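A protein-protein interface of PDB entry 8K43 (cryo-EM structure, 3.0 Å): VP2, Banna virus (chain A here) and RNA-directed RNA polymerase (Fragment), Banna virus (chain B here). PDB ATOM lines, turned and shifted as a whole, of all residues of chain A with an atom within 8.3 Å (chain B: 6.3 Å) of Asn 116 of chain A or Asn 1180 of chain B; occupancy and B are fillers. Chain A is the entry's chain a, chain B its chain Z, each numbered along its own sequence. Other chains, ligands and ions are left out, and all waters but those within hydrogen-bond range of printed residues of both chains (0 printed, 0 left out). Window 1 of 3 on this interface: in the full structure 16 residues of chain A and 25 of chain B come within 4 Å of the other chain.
The backbone NH (N) of Ser 1177 of chain B lies within hydrogen-bond range of the side-chain amide oxygen (OD1) of Asn 116 of chain A. The side-chain amide oxygen (OD1) of Asn 1180 of chain B sits at hydrogen-bond distance from the side-chain amino group (NZ) of Lys 115 of chain A (3.0 Å). OD2 of Asp 119 of chain A is in hydrogen-bond range of ND2 of Asn 1180 of chain B, 2.9 Å away.
OG of Ser 1179 of chain B sits at hydrogen-bond distance from OD1 of Asn 1180 of chain B (3.0 Å). O of Asp 110 of chain A is in hydrogen-bond range of OG1 of Thr 113 of chain A (2.6 Å). OD1 of Asn 117 of chain A lies close to O of Thr 113 of chain A. The side-chain carboxylate (OD2) of Asp 119 of chain A is in salt-bridge range of the side-chain amino group (NZ) of Lys 115 of chain A, 2.5 Å away.
Among the printed residues, merely in contact across the chains: Leu 112 of chain A with Leu 1176 of chain B (3.9 Å), Leu 112 of chain A with Phe 1184 of chain B (3.5 Å), Thr 113 of chain A with Leu 1176 of chain B (3.9 Å), Lys 115 of chain A with Phe 1032 of chain B (3.4 Å), Lys 115 of chain A with Phe 1184 of chain B (3.9 Å), Asn 116 of chain A with Leu 1176 of chain B (3.3 Å) and Asn 116 of chain A with Asn 1180 of chain B (3.4 Å).
Of the printed residues of chain B, Leu 112 of chain A touches Leu 1176 (3.9 Å) and Phe 1184 (3.5 Å). Asn 116 of chain A touches just these residues of chain B: Leu 1176 (3.3 Å), Ser 1177 (3.0 Å) and Asn 1180 (3.4 Å). Of the printed residues of chain B, Asp 119 of chain A touches Asn 1180. Ser 1177 of chain B touches just one residue of chain A: Asn 116 (3.0 Å). No residue of chain A comes within 4 Å of Ser 1179 of chain B. Asn 1180 of chain B touches three residues of chain A. The nearest residue of chain B that does not touch Asn 116 of chain A is Asn 1175 of chain B (4.5 Å). The nearest residue of chain A that does not touch Asn 1180 of chain B is Leu 112 of chain A (5.1 Å).
Hydrophobic or aromatic side chains of chain B that line the printed part of chain A: Phe 1032, Leu 1176 and Phe 1184. Among the printed residues, 10 pairs touch across the chains. Among the printed residues, no Asp or Glu carboxylate lies within 4 Å of a Lys or Arg side-chain nitrogen of the other chain.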
ATOM      1  N   ASP A 110      17.775 -27.869 -12.781  1.00  0.00           N
ATOM      2  CA  ASP A 110      16.357 -27.959 -13.083  1.00  0.00           C
ATOM      3  C   ASP A 110      16.219 -28.385 -14.533  1.00  0.00           C
ATOM      4  O   ASP A 110      17.160 -28.232 -15.320  1.00  0.00           O
ATOM      5  CB  ASP A 110      15.649 -26.617 -12.848  1.00  0.00           C
ATOM      6  CG  ASP A 110      16.428 -25.443 -13.402  1.00  0.00           C
ATOM      7  OD1 ASP A 110      17.437 -25.050 -12.780  1.00  0.00           O
ATOM      8  OD2 ASP A 110      16.036 -24.911 -14.462  1.00  0.00           O
ATOM      9  N   PRO A 111      15.069 -28.945 -14.921  1.00  0.00           N
ATOM     10  CA  PRO A 111      14.934 -29.433 -16.303  1.00  0.00           C
ATOM     11  C   PRO A 111      15.205 -28.369 -17.350  1.00  0.00           C
ATOM     12  O   PRO A 111      15.716 -28.690 -18.431  1.00  0.00           O
ATOM     13  CB  PRO A 111      13.484 -29.937 -16.362  1.00  0.00           C
ATOM     14  CG  PRO A 111      12.825 -29.428 -15.119  1.00  0.00           C
ATOM     15  CD  PRO A 111      13.903 -29.308 -14.104  1.00  0.00           C
ATOM     16  N   LEU A 112      14.892 -27.106 -17.054  1.00  0.00           N
ATOM     17  CA  LEU A 112      15.226 -26.022 -17.972  1.00  0.00           C
ATOM     18  C   LEU A 112      16.733 -25.933 -18.184  1.00  0.00           C
ATOM     19  O   LEU A 112      17.212 -25.878 -19.324  1.00  0.00           O
ATOM     20  CB  LEU A 112      14.681 -24.701 -17.429  1.00  0.00           C
ATOM     21  CG  LEU A 112      13.205 -24.634 -17.047  1.00  0.00           C
ATOM     22  CD1 LEU A 112      12.998 -25.027 -15.597  1.00  0.00           C
ATOM     23  CD2 LEU A 112      12.670 -23.236 -17.289  1.00  0.00           C
ATOM     24  N   THR A 113      17.498 -25.934 -17.092  1.00  0.00           N
ATOM     25  CA  THR A 113      18.948 -25.852 -17.208  1.00  0.00           C
ATOM     26  C   THR A 113      19.535 -27.117 -17.813  1.00  0.00           C
ATOM     27  O   THR A 113      20.536 -27.050 -18.531  1.00  0.00           O
ATOM     28  CB  THR A 113      19.578 -25.579 -15.845  1.00  0.00           C
ATOM     29  OG1 THR A 113      18.931 -26.381 -14.849  1.00  0.00           O
ATOM     30  CG2 THR A 113      19.430 -24.113 -15.479  1.00  0.00           C
ATOM     31  N   ILE A 114      18.934 -28.276 -17.534  1.00  0.00           N
ATOM     32  CA  ILE A 114      19.405 -29.516 -18.143  1.00  0.00           C
ATOM     33  C   ILE A 114      19.245 -29.452 -19.655  1.00  0.00           C
ATOM     34  O   ILE A 114      20.156 -29.812 -20.410  1.00  0.00           O
ATOM     35  CB  ILE A 114      18.664 -30.725 -17.548  1.00  0.00           C
ATOM     36  CG1 ILE A 114      19.007 -30.884 -16.069  1.00  0.00           C
ATOM     37  CG2 ILE A 114      19.016 -31.988 -18.306  1.00  0.00           C
ATOM     38  CD1 ILE A 114      18.101 -31.845 -15.336  1.00  0.00           C
ATOM     39  N   LYS A 115      18.088 -28.979 -20.121  1.00  0.00           N
ATOM     40  CA  LYS A 115      17.880 -28.827 -21.557  1.00  0.00           C
ATOM     41  C   LYS A 115      18.851 -27.815 -22.150  1.00  0.00           C
ATOM     42  O   LYS A 115      19.416 -28.040 -23.227  1.00  0.00           O
ATOM     43  CB  LYS A 115      16.437 -28.416 -21.840  1.00  0.00           C
ATOM     44  CG  LYS A 115      16.261 -27.605 -23.111  1.00  0.00           C
ATOM     45  CD  LYS A 115      16.006 -28.503 -24.303  1.00  0.00           C
ATOM     46  CE  LYS A 115      15.274 -27.761 -25.405  1.00  0.00           C
ATOM     47  NZ  LYS A 115      15.950 -26.484 -25.754  1.00  0.00           N
ATOM     48  N   ASN A 116      19.063 -26.694 -21.457  1.00  0.00           N
ATOM     49  CA  ASN A 116      19.988 -25.686 -21.961  1.00  0.00           C
ATOM     50  C   ASN A 116      21.397 -26.247 -22.099  1.00  0.00           C
ATOM     51  O   ASN A 116      22.069 -26.015 -23.110  1.00  0.00           O
ATOM     52  CB  ASN A 116      19.982 -24.465 -21.043  1.00  0.00           C
ATOM     53  CG  ASN A 116      20.659 -23.266 -21.667  1.00  0.00           C
ATOM     54  OD1 ASN A 116      19.997 -22.333 -22.119  1.00  0.00           O
ATOM     55  ND2 ASN A 116      21.984 -23.278 -21.690  1.00  0.00           N
ATOM     56  N   ASN A 117      21.862 -26.986 -21.091  1.00  0.00           N
ATOM     57  CA  ASN A 117      23.201 -27.560 -21.152  1.00  0.00           C
ATOM     58  C   ASN A 117      23.300 -28.622 -22.237  1.00  0.00           C
ATOM     59  O   ASN A 117      24.308 -28.696 -22.949  1.00  0.00           O
ATOM     60  CB  ASN A 117      23.591 -28.146 -19.793  1.00  0.00           C
ATOM     61  CG  ASN A 117      23.839 -27.080 -18.737  1.00  0.00           C
ATOM     62  OD1 ASN A 117      23.362 -25.954 -18.861  1.00  0.00           O
ATOM     63  ND2 ASN A 117      24.579 -27.432 -17.694  1.00  0.00           N
ATOM     64  N   GLN A 118      22.269 -29.457 -22.379  1.00  0.00           N
ATOM     65  CA  GLN A 118      22.293 -30.494 -23.400  1.00  0.00           C
ATOM     66  C   GLN A 118      22.213 -29.919 -24.805  1.00  0.00           C
ATOM     67  O   GLN A 118      22.639 -30.580 -25.757  1.00  0.00           O
ATOM     68  CB  GLN A 118      21.149 -31.478 -23.175  1.00  0.00           C
ATOM     69  CG  GLN A 118      21.364 -32.409 -22.001  1.00  0.00           C
ATOM     70  CD  GLN A 118      20.441 -33.605 -22.035  1.00  0.00           C
ATOM     71  OE1 GLN A 118      20.866 -34.724 -22.324  1.00  0.00           O
ATOM     72  NE2 GLN A 118      19.168 -33.378 -21.740  1.00  0.00           N
ATOM     73  N   ASP A 119      21.679 -28.707 -24.956  1.00  0.00           N
ATOM     74  CA  ASP A 119      21.624 -28.079 -26.270  1.00  0.00           C
ATOM     75  C   ASP A 119      22.994 -27.664 -26.787  1.00  0.00           C
ATOM     76  O   ASP A 119      23.101 -27.270 -27.953  1.00  0.00           O
ATOM     77  CB  ASP A 119      20.702 -26.860 -26.230  1.00  0.00           C
ATOM     78  CG  ASP A 119      19.235 -27.238 -26.239  1.00  0.00           C
ATOM     79  OD1 ASP A 119      18.931 -28.445 -26.344  1.00  0.00           O
ATOM     80  OD2 ASP A 119      18.385 -26.328 -26.143  1.00  0.00           O
ATOM     81  N   VAL A 120      24.033 -27.738 -25.962  1.00  0.00           N
ATOM     82  CA  VAL A 120      25.357 -27.251 -26.327  1.00  0.00           C
ATOM     83  C   VAL A 120      26.250 -28.368 -26.850  1.00  0.00           C
ATOM     84  O   VAL A 120      26.948 -28.188 -27.848  1.00  0.00           O
ATOM     85  CB  VAL A 120      26.005 -26.538 -25.121  1.00  0.00           C
ATOM     86  CG1 VAL A 120      27.496 -26.371 -25.335  1.00  0.00           C
ATOM     87  CG2 VAL A 120      25.342 -25.192 -24.897  1.00  0.00           C
ATOM     88  N   VAL A 121      26.237 -29.535 -26.201  1.00  0.00           N
ATOM     89  CA  VAL A 121      27.164 -30.603 -26.563  1.00  0.00           C
ATOM     90  C   VAL A 121      26.560 -31.644 -27.494  1.00  0.00           C
ATOM     91  O   VAL A 121      27.307 -32.460 -28.055  1.00  0.00           O
ATOM     92  CB  VAL A 121      27.699 -31.308 -25.304  1.00  0.00           C
ATOM     93  CG1 VAL A 121      28.265 -30.287 -24.333  1.00  0.00           C
ATOM     94  CG2 VAL A 121      26.599 -32.122 -24.648  1.00  0.00           C
ATOM     95  N   ASP A 122      25.243 -31.652 -27.675  1.00  0.00           N
ATOM     96  CA  ASP A 122      24.621 -32.638 -28.547  1.00  0.00           C
ATOM     97  C   ASP A 122      25.030 -32.398 -29.996  1.00  0.00           C
ATOM     98  O   ASP A 122      25.015 -31.261 -30.475  1.00  0.00           O
ATOM     99  CB  ASP A 122      23.102 -32.584 -28.411  1.00  0.00           C
ATOM    100  CG  ASP A 122      22.604 -33.284 -27.162  1.00  0.00           C
ATOM    101  OD1 ASP A 122      23.444 -33.772 -26.378  1.00  0.00           O
ATOM    102  OD2 ASP A 122      21.372 -33.345 -26.963  1.00  0.00           O
ATOM    103  N   GLN A 146      30.138 -31.256 -17.670  1.00  0.00           N
ATOM    104  CA  GLN A 146      29.063 -30.321 -17.364  1.00  0.00           C
ATOM    105  C   GLN A 146      28.042 -30.880 -16.382  1.00  0.00           C
ATOM    106  O   GLN A 146      27.224 -30.111 -15.866  1.00  0.00           O
ATOM    107  CB  GLN A 146      28.360 -29.880 -18.648  1.00  0.00           C
ATOM    108  CG  GLN A 146      27.422 -30.911 -19.236  1.00  0.00           C
ATOM    109  CD  GLN A 146      26.843 -30.470 -20.565  1.00  0.00           C
ATOM    110  OE1 GLN A 146      27.103 -29.361 -21.030  1.00  0.00           O
ATOM    111  NE2 GLN A 146      26.054 -31.339 -21.184  1.00  0.00           N
ATOM    112  N   PHE A 147      28.065 -32.180 -16.109  1.00  0.00           N
ATOM    113  CA  PHE A 147      27.166 -32.768 -15.119  1.00  0.00           C
ATOM    114  C   PHE A 147      27.943 -33.564 -14.079  1.00  0.00           C
ATOM    115  O   PHE A 147      28.650 -32.998 -13.248  1.00  0.00           O
ATOM    116  CB  PHE A 147      26.126 -33.666 -15.789  1.00  0.00           C
ATOM    117  CG  PHE A 147      25.117 -32.922 -16.609  1.00  0.00           C
ATOM    118  CD1 PHE A 147      24.252 -32.024 -16.016  1.00  0.00           C
ATOM    119  CD2 PHE A 147      25.024 -33.135 -17.972  1.00  0.00           C
ATOM    120  CE1 PHE A 147      23.320 -31.343 -16.766  1.00  0.00           C
ATOM    121  CE2 PHE A 147      24.093 -32.454 -18.728  1.00  0.00           C
ATOM    122  CZ  PHE A 147      23.240 -31.558 -18.124  1.00  0.00           C
ATOM    123  N   PHE B1032      10.327 -29.309 -25.710  1.00  0.00           N
ATOM    124  CA  PHE B1032      10.235 -28.626 -24.429  1.00  0.00           C
ATOM    125  C   PHE B1032       9.224 -29.328 -23.537  1.00  0.00           C
ATOM    126  O   PHE B1032       8.158 -29.743 -23.997  1.00  0.00           O
ATOM    127  CB  PHE B1032       9.834 -27.163 -24.611  1.00  0.00           C
ATOM    128  CG  PHE B1032      10.909 -26.316 -25.219  1.00  0.00           C
ATOM    129  CD1 PHE B1032      11.940 -25.825 -24.445  1.00  0.00           C
ATOM    130  CD2 PHE B1032      10.891 -26.016 -26.567  1.00  0.00           C
ATOM    131  CE1 PHE B1032      12.931 -25.047 -25.002  1.00  0.00           C
ATOM    132  CE2 PHE B1032      11.876 -25.239 -27.129  1.00  0.00           C
ATOM    133  CZ  PHE B1032      12.898 -24.755 -26.347  1.00  0.00           C
ATOM    134  N   HIS B1138      12.798 -21.950 -30.953  1.00  0.00           N
ATOM    135  CA  HIS B1138      11.801 -22.605 -30.113  1.00  0.00           C
ATOM    136  C   HIS B1138      10.503 -22.830 -30.872  1.00  0.00           C
ATOM    137  O   HIS B1138       9.879 -23.890 -30.745  1.00  0.00           O
ATOM    138  CB  HIS B1138      11.540 -21.775 -28.859  1.00  0.00           C
ATOM    139  CG  HIS B1138      10.973 -20.420 -29.140  1.00  0.00           C
ATOM    140  ND1 HIS B1138       9.624 -20.150 -29.068  1.00  0.00           N
ATOM    141  CD2 HIS B1138      11.570 -19.258 -29.492  1.00  0.00           C
ATOM    142  CE1 HIS B1138       9.416 -18.879 -29.365  1.00  0.00           C
ATOM    143  NE2 HIS B1138      10.580 -18.316 -29.627  1.00  0.00           N
ATOM    144  N   ILE B1172      10.956 -17.066 -14.194  1.00  0.00           N
ATOM    145  CA  ILE B1172      12.091 -17.926 -14.504  1.00  0.00           C
ATOM    146  C   ILE B1172      13.351 -17.196 -14.070  1.00  0.00           C
ATOM    147  O   ILE B1172      13.633 -16.094 -14.556  1.00  0.00           O
ATOM    148  CB  ILE B1172      12.151 -18.279 -15.996  1.00  0.00           C
ATOM    149  CG1 ILE B1172      10.893 -19.032 -16.419  1.00  0.00           C
ATOM    150  CG2 ILE B1172      13.390 -19.105 -16.294  1.00  0.00           C
ATOM    151  CD1 ILE B1172      10.961 -19.591 -17.819  1.00  0.00           C
ATOM    152  N   ASN B1175      19.544 -18.905 -15.863  1.00  0.00           N
ATOM    153  CA  ASN B1175      20.179 -18.253 -17.002  1.00  0.00           C
ATOM    154  C   ASN B1175      20.118 -19.192 -18.201  1.00  0.00           C
ATOM    155  O   ASN B1175      20.814 -20.212 -18.237  1.00  0.00           O
ATOM    156  CB  ASN B1175      21.618 -17.873 -16.668  1.00  0.00           C
ATOM    157  CG  ASN B1175      22.342 -18.961 -15.905  1.00  0.00           C
ATOM    158  OD1 ASN B1175      21.965 -19.305 -14.785  1.00  0.00           O
ATOM    159  ND2 ASN B1175      23.390 -19.511 -16.509  1.00  0.00           N
ATOM    160  N   LEU B1176      19.289 -18.845 -19.184  1.00  0.00           N
ATOM    161  CA  LEU B1176      19.080 -19.666 -20.364  1.00  0.00           C
ATOM    162  C   LEU B1176      19.165 -18.799 -21.610  1.00  0.00           C
ATOM    163  O   LEU B1176      19.008 -17.576 -21.553  1.00  0.00           O
ATOM    164  CB  LEU B1176      17.719 -20.377 -20.322  1.00  0.00           C
ATOM    165  CG  LEU B1176      17.262 -20.957 -18.987  1.00  0.00           C
ATOM    166  CD1 LEU B1176      15.809 -21.388 -19.070  1.00  0.00           C
ATOM    167  CD2 LEU B1176      18.142 -22.125 -18.581  1.00  0.00           C
ATOM    168  N   SER B1177      19.419 -19.446 -22.743  1.00  0.00           N
ATOM    169  CA  SER B1177      19.428 -18.749 -24.018  1.00  0.00           C
ATOM    170  C   SER B1177      18.019 -18.296 -24.388  1.00  0.00           C
ATOM    171  O   SER B1177      17.021 -18.768 -23.838  1.00  0.00           O
ATOM    172  CB  SER B1177      19.997 -19.643 -25.116  1.00  0.00           C
ATOM    173  OG  SER B1177      18.958 -20.266 -25.849  1.00  0.00           O
ATOM    174  N   ASN B1178      17.949 -17.363 -25.339  1.00  0.00           N
ATOM    175  CA  ASN B1178      16.679 -16.715 -25.654  1.00  0.00           C
ATOM    176  C   ASN B1178      15.652 -17.708 -26.185  1.00  0.00           C
ATOM    177  O   ASN B1178      14.473 -17.646 -25.817  1.00  0.00           O
ATOM    178  CB  ASN B1178      16.903 -15.589 -26.660  1.00  0.00           C
ATOM    179  CG  ASN B1178      17.850 -14.532 -26.145  1.00  0.00           C
ATOM    180  OD1 ASN B1178      18.119 -14.456 -24.947  1.00  0.00           O
ATOM    181  ND2 ASN B1178      18.365 -13.706 -27.047  1.00  0.00           N
ATOM    182  N   SER B1179      16.076 -18.627 -27.056  1.00  0.00           N
ATOM    183  CA  SER B1179      15.140 -19.596 -27.617  1.00  0.00           C
ATOM    184  C   SER B1179      14.571 -20.501 -26.533  1.00  0.00           C
ATOM    185  O   SER B1179      13.352 -20.703 -26.448  1.00  0.00           O
ATOM    186  CB  SER B1179      15.832 -20.419 -28.701  1.00  0.00           C
ATOM    187  OG  SER B1179      16.372 -21.611 -28.161  1.00  0.00           O
ATOM    188  N   ASN B1180      15.443 -21.058 -25.690  1.00  0.00           N
ATOM    189  CA  ASN B1180      14.978 -21.916 -24.606  1.00  0.00           C
ATOM    190  C   ASN B1180      14.112 -21.138 -23.627  1.00  0.00           C
ATOM    191  O   ASN B1180      13.094 -21.650 -23.142  1.00  0.00           O
ATOM    192  CB  ASN B1180      16.172 -22.542 -23.889  1.00  0.00           C
ATOM    193  CG  ASN B1180      16.902 -23.547 -24.750  1.00  0.00           C
ATOM    194  OD1 ASN B1180      16.684 -23.620 -25.957  1.00  0.00           O
ATOM    195  ND2 ASN B1180      17.776 -24.330 -24.133  1.00  0.00           N
ATOM    196  N   ARG B1181      14.499 -19.896 -23.330  1.00  0.00           N
ATOM    197  CA  ARG B1181      13.710 -19.072 -22.424  1.00  0.00           C
ATOM    198  C   ARG B1181      12.304 -18.852 -22.963  1.00  0.00           C
ATOM    199  O   ARG B1181      11.321 -18.987 -22.224  1.00  0.00           O
ATOM    200  CB  ARG B1181      14.408 -17.733 -22.197  1.00  0.00           C
ATOM    201  CG  ARG B1181      13.631 -16.780 -21.317  1.00  0.00           C
ATOM    202  CD  ARG B1181      14.506 -15.653 -20.822  1.00  0.00           C
ATOM    203  NE  ARG B1181      13.894 -14.948 -19.705  1.00  0.00           N
ATOM    204  CZ  ARG B1181      14.238 -15.118 -18.435  1.00  0.00           C
ATOM    205  NH1 ARG B1181      15.194 -15.962 -18.088  1.00  0.00           N
ATOM    206  NH2 ARG B1181      13.609 -14.423 -17.493  1.00  0.00           N
ATOM    207  N   ARG B1182      12.185 -18.530 -24.252  1.00  0.00           N
ATOM    208  CA  ARG B1182      10.864 -18.304 -24.827  1.00  0.00           C
ATOM    209  C   ARG B1182      10.051 -19.590 -24.866  1.00  0.00           C
ATOM    210  O   ARG B1182       8.838 -19.575 -24.613  1.00  0.00           O
ATOM    211  CB  ARG B1182      10.995 -17.701 -26.223  1.00  0.00           C
ATOM    212  CG  ARG B1182      10.778 -16.197 -26.255  1.00  0.00           C
ATOM    213  CD  ARG B1182      11.127 -15.608 -27.610  1.00  0.00           C
ATOM    214  NE  ARG B1182      10.013 -15.682 -28.546  1.00  0.00           N
ATOM    215  CZ  ARG B1182      10.035 -15.192 -29.778  1.00  0.00           C
ATOM    216  NH1 ARG B1182      11.107 -14.587 -30.261  1.00  0.00           N
ATOM    217  NH2 ARG B1182       8.955 -15.313 -30.545  1.00  0.00           N
ATOM    218  N   GLY B1183      10.695 -20.715 -25.179  1.00  0.00           N
ATOM    219  CA  GLY B1183       9.974 -21.977 -25.167  1.00  0.00           C
ATOM    220  C   GLY B1183       9.406 -22.299 -23.800  1.00  0.00           C
ATOM    221  O   GLY B1183       8.235 -22.671 -23.671  1.00  0.00           O
ATOM    222  N   PHE B1184      10.213 -22.124 -22.757  1.00  0.00           N
ATOM    223  CA  PHE B1184       9.721 -22.398 -21.415  1.00  0.00           C
ATOM    224  C   PHE B1184       8.680 -21.374 -20.985  1.00  0.00           C
ATOM    225  O   PHE B1184       7.784 -21.696 -20.195  1.00  0.00           O
ATOM    226  CB  PHE B1184      10.890 -22.454 -20.441  1.00  0.00           C
ATOM    227  CG  PHE B1184      11.781 -23.638 -20.654  1.00  0.00           C
ATOM    228  CD1 PHE B1184      11.245 -24.905 -20.762  1.00  0.00           C
ATOM    229  CD2 PHE B1184      13.151 -23.486 -20.761  1.00  0.00           C
ATOM    230  CE1 PHE B1184      12.051 -25.996 -20.965  1.00  0.00           C
ATOM    231  CE2 PHE B1184      13.966 -24.578 -20.966  1.00  0.00           C
ATOM    232  CZ  PHE B1184      13.413 -25.836 -21.068  1.00  0.00           C
ATOM    233  N   GLN B1185       8.759 -20.151 -21.507  1.00  0.00           N
ATOM    234  CA  GLN B1185       7.724 -19.167 -21.210  1.00  0.00           C
ATOM    235  C   GLN B1185       6.380 -19.575 -21.805  1.00  0.00           C
ATOM    236  O   GLN B1185       5.344 -19.440 -21.147  1.00  0.00           O
ATOM    237  CB  GLN B1185       8.155 -17.789 -21.706  1.00  0.00           C
ATOM    238  CG  GLN B1185       8.960 -17.017 -20.673  1.00  0.00           C
ATOM    239  CD  GLN B1185       9.611 -15.775 -21.235  1.00  0.00           C
ATOM    240  OE1 GLN B1185      10.221 -15.809 -22.303  1.00  0.00           O
ATOM    241  NE2 GLN B1185       9.493 -14.670 -20.512  1.00  0.00           N
